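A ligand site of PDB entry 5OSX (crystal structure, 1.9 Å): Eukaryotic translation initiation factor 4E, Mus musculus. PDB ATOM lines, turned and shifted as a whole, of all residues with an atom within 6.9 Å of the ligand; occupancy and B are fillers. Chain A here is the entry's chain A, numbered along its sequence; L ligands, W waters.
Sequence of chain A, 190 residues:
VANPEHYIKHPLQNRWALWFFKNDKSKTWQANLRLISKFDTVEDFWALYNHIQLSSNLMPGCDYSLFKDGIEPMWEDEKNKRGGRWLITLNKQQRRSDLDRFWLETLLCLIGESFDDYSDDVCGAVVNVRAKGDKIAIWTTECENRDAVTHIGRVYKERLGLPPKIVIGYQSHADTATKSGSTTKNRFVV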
ATOM      1  N   PHE A  21       2.624  24.125  10.506  1.00  0.00           N
ATOM      2  CA  PHE A  21       3.354  25.383  10.437  1.00  0.00           C
ATOM      3  C   PHE A  21       4.261  25.358   9.211  1.00  0.00           C
ATOM      4  O   PHE A  21       4.908  24.346   8.945  1.00  0.00           O
ATOM      5  CB  PHE A  21       4.186  25.636  11.723  1.00  0.00           C
ATOM      6  CG  PHE A  21       5.095  26.850  11.640  1.00  0.00           C
ATOM      7  CD1 PHE A  21       4.692  28.040  12.215  1.00  0.00           C
ATOM      8  CD2 PHE A  21       6.330  26.784  11.029  1.00  0.00           C
ATOM      9  CE1 PHE A  21       5.514  29.159  12.138  1.00  0.00           C
ATOM     10  CE2 PHE A  21       7.143  27.892  10.972  1.00  0.00           C
ATOM     11  CZ  PHE A  21       6.733  29.071  11.518  1.00  0.00           C
ATOM     12  N   ASN A  23       7.311  27.812   7.425  1.00  0.00           N
ATOM     13  CA  ASN A  23       8.172  28.989   7.573  1.00  0.00           C
ATOM     14  C   ASN A  23       8.054  29.852   6.325  1.00  0.00           C
ATOM     15  O   ASN A  23       8.894  29.815   5.420  1.00  0.00           O
ATOM     16  CB  ASN A  23       9.617  28.565   7.805  1.00  0.00           C
ATOM     17  CG  ASN A  23      10.315  29.415   8.837  1.00  0.00           C
ATOM     18  OD1 ASN A  23       9.890  30.538   9.130  1.00  0.00           O
ATOM     19  ND2 ASN A  23      11.395  28.885   9.417  1.00  0.00           N
ATOM     20  N   TRP A  29       5.266  34.621  12.775  1.00  0.00           N
ATOM     21  CA  TRP A  29       5.248  33.217  13.190  1.00  0.00           C
ATOM     22  C   TRP A  29       3.833  32.742  13.452  1.00  0.00           C
ATOM     23  O   TRP A  29       3.456  31.629  13.048  1.00  0.00           O
ATOM     24  CB  TRP A  29       6.106  33.015  14.435  1.00  0.00           C
ATOM     25  CG  TRP A  29       6.221  31.572  14.837  1.00  0.00           C
ATOM     26  CD1 TRP A  29       7.122  30.671  14.374  1.00  0.00           C
ATOM     27  CD2 TRP A  29       5.392  30.870  15.773  1.00  0.00           C
ATOM     28  NE1 TRP A  29       6.906  29.443  14.972  1.00  0.00           N
ATOM     29  CE2 TRP A  29       5.861  29.543  15.842  1.00  0.00           C
ATOM     30  CE3 TRP A  29       4.310  31.243  16.582  1.00  0.00           C
ATOM     31  CZ2 TRP A  29       5.269  28.575  16.677  1.00  0.00           C
ATOM     32  CZ3 TRP A  29       3.731  30.288  17.405  1.00  0.00           C
ATOM     33  CH2 TRP A  29       4.213  28.966  17.442  1.00  0.00           C
ATOM     34  N   GLN A  30       3.020  33.561  14.123  1.00  0.00           N
ATOM     35  CA  GLN A  30       1.696  33.079  14.535  1.00  0.00           C
ATOM     36  C   GLN A  30       0.769  32.919  13.331  1.00  0.00           C
ATOM     37  O   GLN A  30      -0.023  31.969  13.273  1.00  0.00           O
ATOM     38  CB  GLN A  30       1.091  34.009  15.567  1.00  0.00           C
ATOM     39  N   GLY A  61      11.721  23.331   7.925  1.00  0.00           N
ATOM     40  CA  GLY A  61      11.053  24.506   8.402  1.00  0.00           C
ATOM     41  C   GLY A  61       9.585  24.302   8.759  1.00  0.00           C
ATOM     42  O   GLY A  61       8.978  25.222   9.325  1.00  0.00           O
ATOM     43  N   ASP A  63       6.346  22.386  10.797  1.00  0.00           N
ATOM     44  CA  ASP A  63       6.040  21.674  12.014  1.00  0.00           C
ATOM     45  C   ASP A  63       4.691  20.997  11.867  1.00  0.00           C
ATOM     46  O   ASP A  63       3.785  21.518  11.194  1.00  0.00           O
ATOM     47  CB  ASP A  63       5.946  22.551  13.275  1.00  0.00           C
ATOM     48  CG  ASP A  63       7.139  23.464  13.468  1.00  0.00           C
ATOM     49  OD1 ASP A  63       8.269  23.095  13.098  1.00  0.00           O
ATOM     50  OD2 ASP A  63       6.917  24.573  14.025  1.00  0.00           O
ATOM     51  N   PRO A  73      -0.867  25.672  20.169  1.00  0.00           N
ATOM     52  CA  PRO A  73       0.496  25.116  20.305  1.00  0.00           C
ATOM     53  C   PRO A  73       1.564  26.198  20.375  1.00  0.00           C
ATOM     54  O   PRO A  73       2.517  26.199  19.583  1.00  0.00           O
ATOM     55  CB  PRO A  73       0.627  24.239  19.070  1.00  0.00           C
ATOM     56  CG  PRO A  73      -0.204  24.926  18.042  1.00  0.00           C
ATOM     57  CD  PRO A  73      -1.372  25.523  18.798  1.00  0.00           C
ATOM     58  N   MET A  74       1.403  27.125  21.302  1.00  0.00           N
ATOM     59  CA  MET A  74       2.387  28.176  21.492  1.00  0.00           C
ATOM     60  C   MET A  74       2.593  28.400  22.979  1.00  0.00           C
ATOM     61  O   MET A  74       1.677  28.163  23.786  1.00  0.00           O
ATOM     62  CB  MET A  74       2.004  29.486  20.784  1.00  0.00           C
ATOM     63  CG  MET A  74       0.683  30.085  21.188  1.00  0.00           C
ATOM     64  SD  MET A  74       0.040  31.105  19.849  1.00  0.00           S
ATOM     65  CE  MET A  74       0.163  29.926  18.506  1.00  0.00           C
ATOM     66  N   TRP A  75       3.797  28.849  23.324  1.00  0.00           N
ATOM     67  CA  TRP A  75       4.129  29.167  24.708  1.00  0.00           C
ATOM     68  C   TRP A  75       3.103  30.091  25.351  1.00  0.00           C
ATOM     69  O   TRP A  75       2.966  30.099  26.577  1.00  0.00           O
ATOM     70  CB  TRP A  75       5.481  29.874  24.798  1.00  0.00           C
ATOM     71  CG  TRP A  75       6.611  29.195  24.111  1.00  0.00           C
ATOM     72  CD1 TRP A  75       6.963  27.884  24.201  1.00  0.00           C
ATOM     73  CD2 TRP A  75       7.600  29.817  23.266  1.00  0.00           C
ATOM     74  NE1 TRP A  75       8.093  27.636  23.449  1.00  0.00           N
ATOM     75  CE2 TRP A  75       8.506  28.820  22.873  1.00  0.00           C
ATOM     76  CE3 TRP A  75       7.794  31.123  22.817  1.00  0.00           C
ATOM     77  CZ2 TRP A  75       9.586  29.084  22.043  1.00  0.00           C
ATOM     78  CZ3 TRP A  75       8.869  31.385  21.979  1.00  0.00           C
ATOM     79  CH2 TRP A  75       9.745  30.368  21.597  1.00  0.00           C
ATOM     80  N   GLU A  76       2.414  30.906  24.552  1.00  0.00           N
ATOM     81  CA  GLU A  76       1.582  31.973  25.098  1.00  0.00           C
ATOM     82  C   GLU A  76       0.296  31.442  25.704  1.00  0.00           C
ATOM     83  O   GLU A  76      -0.293  32.124  26.538  1.00  0.00           O
ATOM     84  CB  GLU A  76       1.246  32.998  24.014  1.00  0.00           C
ATOM     85  CG  GLU A  76       2.347  34.024  23.718  1.00  0.00           C
ATOM     86  CD  GLU A  76       3.456  33.508  22.821  1.00  0.00           C
ATOM     87  OE1 GLU A  76       4.399  34.283  22.566  1.00  0.00           O
ATOM     88  OE2 GLU A  76       3.408  32.318  22.391  1.00  0.00           O
ATOM     89  N   ASN A  80       0.246  26.478  28.501  1.00  0.00           N
ATOM     90  CA  ASN A  80       1.648  26.248  28.203  1.00  0.00           C
ATOM     91  C   ASN A  80       2.589  27.194  28.952  1.00  0.00           C
ATOM     92  O   ASN A  80       3.767  26.855  29.121  1.00  0.00           O
ATOM     93  CB  ASN A  80       1.908  26.358  26.678  1.00  0.00           C
ATOM     94  CG  ASN A  80       1.100  25.348  25.840  1.00  0.00           C
ATOM     95  OD1 ASN A  80       0.914  24.181  26.247  1.00  0.00           O
ATOM     96  ND2 ASN A  80       0.656  25.773  24.655  1.00  0.00           N
ATOM     97  N   ARG A  85       8.748  21.259  27.998  1.00  0.00           N
ATOM     98  CA  ARG A  85       8.668  20.190  27.015  1.00  0.00           C
ATOM     99  C   ARG A  85       9.743  19.158  27.260  1.00  0.00           C
ATOM    100  O   ARG A  85      10.860  19.476  27.681  1.00  0.00           O
ATOM    101  CB  ARG A  85       8.795  20.743  25.577  1.00  0.00           C
ATOM    102  CG  ARG A  85      10.151  21.354  25.292  1.00  0.00           C
ATOM    103  CD  ARG A  85      10.331  21.730  23.808  1.00  0.00           C
ATOM    104  NE  ARG A  85      11.615  22.381  23.557  1.00  0.00           N
ATOM    105  CZ  ARG A  85      12.013  22.825  22.377  1.00  0.00           C
ATOM    106  NH1 ARG A  85      11.237  22.682  21.292  1.00  0.00           N
ATOM    107  NH2 ARG A  85      13.195  23.424  22.262  1.00  0.00           N
ATOM    108  N   VAL A 126       4.883  18.327  19.438  1.00  0.00           N
ATOM    109  CA  VAL A 126       5.362  19.101  18.303  1.00  0.00           C
ATOM    110  C   VAL A 126       6.508  18.345  17.662  1.00  0.00           C
ATOM    111  O   VAL A 126       7.423  17.897  18.347  1.00  0.00           O
ATOM    112  CB  VAL A 126       5.833  20.509  18.715  1.00  0.00           C
ATOM    113  CG1 VAL A 126       6.343  21.286  17.512  1.00  0.00           C
ATOM    114  CG2 VAL A 126       4.725  21.273  19.427  1.00  0.00           C
ATOM    115  N   ASN A 128       9.396  19.317  14.811  1.00  0.00           N
ATOM    116  CA  ASN A 128      10.014  20.317  13.940  1.00  0.00           C
ATOM    117  C   ASN A 128      10.897  19.595  12.936  1.00  0.00           C
ATOM    118  O   ASN A 128      11.797  18.855  13.333  1.00  0.00           O
ATOM    119  CB  ASN A 128      10.865  21.335  14.702  1.00  0.00           C
ATOM    120  CG  ASN A 128      10.204  21.852  15.948  1.00  0.00           C
ATOM    121  OD1 ASN A 128      10.615  21.534  17.066  1.00  0.00           O
ATOM    122  ND2 ASN A 128       9.186  22.687  15.768  1.00  0.00           N
ATOM    123  N   VAL A 129      10.618  19.795  11.659  1.00  0.00           N
ATOM    124  CA  VAL A 129      11.466  19.309  10.590  1.00  0.00           C
ATOM    125  C   VAL A 129      12.400  20.460  10.268  1.00  0.00           C
ATOM    126  O   VAL A 129      11.924  21.566   9.971  1.00  0.00           O
ATOM    127  CB  VAL A 129      10.634  18.890   9.371  1.00  0.00           C
ATOM    128  CG1 VAL A 129      11.492  18.286   8.279  1.00  0.00           C
ATOM    129  CG2 VAL A 129       9.536  17.913   9.798  1.00  0.00           C
ATOM    130  N   ARG A 130      13.711  20.225  10.387  1.00  0.00           N
ATOM    131  CA  ARG A 130      14.732  21.254  10.260  1.00  0.00           C
ATOM    132  C   ARG A 130      15.966  20.706   9.559  1.00  0.00           C
ATOM    133  O   ARG A 130      16.438  19.607   9.892  1.00  0.00           O
ATOM    134  CB  ARG A 130      15.154  21.819  11.621  1.00  0.00           C
ATOM    135  CG  ARG A 130      14.057  22.535  12.386  1.00  0.00           C
ATOM    136  CD  ARG A 130      13.556  23.767  11.651  1.00  0.00           C
ATOM    137  NE  ARG A 130      12.585  24.489  12.469  1.00  0.00           N
ATOM    138  CZ  ARG A 130      11.281  24.220  12.488  1.00  0.00           C
ATOM    139  NH1 ARG A 130      10.788  23.237  11.761  1.00  0.00           N
ATOM    140  NH2 ARG A 130      10.475  24.937  13.266  1.00  0.00           N
ATOM    141  N   LYS A 132      18.766  21.621  10.194  1.00  0.00           N
ATOM    142  CA  LYS A 132      19.781  21.538  11.239  1.00  0.00           C
ATOM    143  C   LYS A 132      19.628  20.318  12.122  1.00  0.00           C
ATOM    144  O   LYS A 132      20.494  20.090  12.971  1.00  0.00           O
ATOM    145  CB  LYS A 132      19.751  22.797  12.107  1.00  0.00           C
ATOM    146  N   GLY A 133      18.542  19.554  11.980  1.00  0.00           N
ATOM    147  CA  GLY A 133      18.292  18.409  12.830  1.00  0.00           C
ATOM    148  C   GLY A 133      16.862  18.458  13.337  1.00  0.00           C
ATOM    149  O   GLY A 133      16.455  19.487  13.884  1.00  0.00           O
ATOM    150  N   LYS A 135      13.323  17.628  15.529  1.00  0.00           N
ATOM    151  CA  LYS A 135      13.016  17.612  16.950  1.00  0.00           C
ATOM    152  C   LYS A 135      11.577  17.172  17.121  1.00  0.00           C
ATOM    153  O   LYS A 135      10.700  17.518  16.319  1.00  0.00           O
ATOM    154  CB  LYS A 135      13.231  18.993  17.587  1.00  0.00           C
ATOM    155  CG  LYS A 135      14.692  19.350  17.821  1.00  0.00           C
ATOM    156  CD  LYS A 135      14.851  20.747  18.429  1.00  0.00           C
ATOM    157  CE  LYS A 135      14.690  21.818  17.370  1.00  0.00           C
ATOM    158  NZ  LYS A 135      14.606  23.209  17.912  1.00  0.00           N
ATOM    159  N   TRP A 139       4.745  18.590  25.121  1.00  0.00           N
ATOM    160  CA  TRP A 139       4.538  19.734  25.984  1.00  0.00           C
ATOM    161  C   TRP A 139       3.597  19.379  27.138  1.00  0.00           C
ATOM    162  O   TRP A 139       2.524  18.809  26.926  1.00  0.00           O
ATOM    163  CB  TRP A 139       3.947  20.899  25.189  1.00  0.00           C
ATOM    164  CG  TRP A 139       4.851  21.469  24.147  1.00  0.00           C
ATOM    165  CD1 TRP A 139       5.926  20.861  23.548  1.00  0.00           C
ATOM    166  CD2 TRP A 139       4.772  22.780  23.612  1.00  0.00           C
ATOM    167  NE1 TRP A 139       6.503  21.731  22.640  1.00  0.00           N
ATOM    168  CE2 TRP A 139       5.822  22.923  22.675  1.00  0.00           C
ATOM    169  CE3 TRP A 139       3.929  23.867  23.847  1.00  0.00           C
ATOM    170  CZ2 TRP A 139       6.026  24.098  21.954  1.00  0.00           C
ATOM    171  CZ3 TRP A 139       4.127  25.040  23.142  1.00  0.00           C
ATOM    172  CH2 TRP A 139       5.174  25.143  22.193  1.00  0.00           C
ATOM    173  N   THR A 176      13.088  28.604  27.399  1.00  0.00           N
ATOM    174  CA  THR A 176      13.008  28.627  25.938  1.00  0.00           C
ATOM    175  C   THR A 176      12.242  29.852  25.440  1.00  0.00           C
ATOM    176  O   THR A 176      12.740  30.632  24.628  1.00  0.00           O
ATOM    177  CB  THR A 176      12.316  27.349  25.375  1.00  0.00           C
ATOM    178  OG1 THR A 176      12.995  26.174  25.842  1.00  0.00           O
ATOM    179  CG2 THR A 176      12.320  27.351  23.856  1.00  0.00           C
HETATM  180  S1  LIG L   1      17.607  26.653  16.848  1.00  0.00           S
HETATM  181  P1  LIG L   1      11.412  26.466  17.054  1.00  0.00           P
HETATM  182  O1  LIG L   1      10.613  26.553  15.803  1.00  0.00           O
HETATM  183  O2  LIG L   1      10.725  25.693  18.113  1.00  0.00           O
HETATM  184  O3  LIG L   1      12.790  25.659  16.886  1.00  0.00           O
HETATM  185  P2  LIG L   1      13.873  26.031  15.749  1.00  0.00           P
HETATM  186  O4  LIG L   1      13.331  26.134  14.371  1.00  0.00           O
HETATM  187  O5  LIG L   1      14.882  24.956  15.853  1.00  0.00           O
HETATM  188  O6  LIG L   1      14.650  27.365  16.245  1.00  0.00           O
HETATM  189  P3  LIG L   1      15.729  27.265  17.447  1.00  0.00           P
HETATM  190  O7  LIG L   1      15.721  28.597  18.115  1.00  0.00           O
HETATM  191  O8  LIG L   1      15.136  26.337  18.440  1.00  0.00           O
HETATM  192  S2  LIG L   1      11.872  28.328  17.932  1.00  0.00           S
HETATM  193  C1  LIG L   1      12.146  29.410  16.470  1.00  0.00           C
HETATM  194  C2  LIG L   1      11.306  30.706  16.492  1.00  0.00           C
HETATM  195  O9  LIG L   1       9.914  30.413  16.247  1.00  0.00           O
HETATM  196  C3  LIG L   1      11.278  31.360  17.867  1.00  0.00           C
HETATM  197  O10 LIG L   1      12.504  32.075  18.103  1.00  0.00           O
HETATM  198  C4  LIG L   1      10.129  32.319  17.710  1.00  0.00           C
HETATM  199  O11 LIG L   1      10.445  33.382  16.780  1.00  0.00           O
HETATM  200  C5  LIG L   1       9.134  31.361  17.069  1.00  0.00           C
HETATM  201  N1  LIG L   1       8.339  30.536  18.015  1.00  0.00           N
HETATM  202  C6  LIG L   1       8.444  29.244  18.240  1.00  0.00           C
HETATM  203  N2  LIG L   1       7.521  28.907  19.149  1.00  0.00           N
HETATM  204  C7  LIG L   1       7.400  27.509  19.602  1.00  0.00           C
HETATM  205  C8  LIG L   1       6.845  30.001  19.496  1.00  0.00           C
HETATM  206  C9  LIG L   1       7.367  31.013  18.778  1.00  0.00           C
HETATM  207  N3  LIG L   1       6.896  32.266  18.897  1.00  0.00           N
HETATM  208  C10 LIG L   1       5.875  32.513  19.750  1.00  0.00           C
HETATM  209  N4  LIG L   1       5.378  33.734  19.905  1.00  0.00           N
HETATM  210  N5  LIG L   1       5.366  31.499  20.473  1.00  0.00           N
HETATM  211  C11 LIG L   1       5.830  30.265  20.341  1.00  0.00           C
HETATM  212  O12 LIG L   1       5.283  29.268  21.095  1.00  0.00           O
HETATM  213  O   HOH W   1      10.277  28.279  13.309  1.00  0.00           O
HETATM  214  O   HOH W   2       7.184  34.800  17.588  1.00  0.00           O
HETATM  215  O   HOH W   3       8.199  26.791  14.677  1.00  0.00           O
HETATM  216  O   HOH W   4       8.663  24.256  19.060  1.00  0.00           O
HETATM  217  O   HOH W   5      14.111  25.215  20.484  1.00  0.00           O
HETATM  218  O   HOH W   6      11.990  23.351  18.680  1.00  0.00           O
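CA of Met 74 touches O12 of the ligand (3.1 Å). Hydrophobic or aromatic side chains within 4 Å of the ligand: Trp 29, Met 74 and Trp 75.
Water W5 lies within hydrogen-bond range of O8 of the ligand (2.5 Å), NH2 of Arg 85 (2.7 Å) and NZ of Lys 135 (3.3 Å). Water W3 lies within hydrogen-bond range of the side-chain carboxylate (OD2) of Asp 63 (2.6 Å), an oxygen (O1) of the ligand (2.7 Å), the indole nitrogen (NE1) of Trp 29 (3.0 Å) and the guanidinium group (NH2) of Arg 130 (3.3 Å). Water W6 lies within hydrogen-bond range of an oxygen (O2) of the ligand (2.7 Å), the side-chain amino group (NZ) of Lys 135 (2.7 Å), the side-chain amide oxygen (OD1) of Asn 128 (2.8 Å) and the guanidinium group (NH1) of Arg 85 (2.8 Å). Water W1 bridges an oxygen (O1) of the ligand (3.1 Å) and the guanidinium group (NH2) of Arg 130 (3.3 Å).
NH1 of Arg 130 is in salt-bridge range of OD1 of Asp 63 (2.9 Å). The backbone NH of Asn 128 is in hydrogen-bond range of the backbone carbonyl oxygen of Lys 135 (2.7 Å). O of Met 74 lies within hydrogen-bond range of ND2 of Asn 80.
NE of Arg 130 lies within salt-bridge range of O4 of the ligand, at 2.6 Å. N of Trp 75 lies within hydrogen-bond range of O12 of the ligand. NZ of Lys 135 is in salt-bridge range of O5 of the ligand (2.7 Å). The side-chain carboxylate (OE2) of Glu 76 is in hydrogen-bond range of a nitrogen (N5) of the ligand. O9 of the ligand sits close to NE1 of Trp 29 (3.4 Å).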
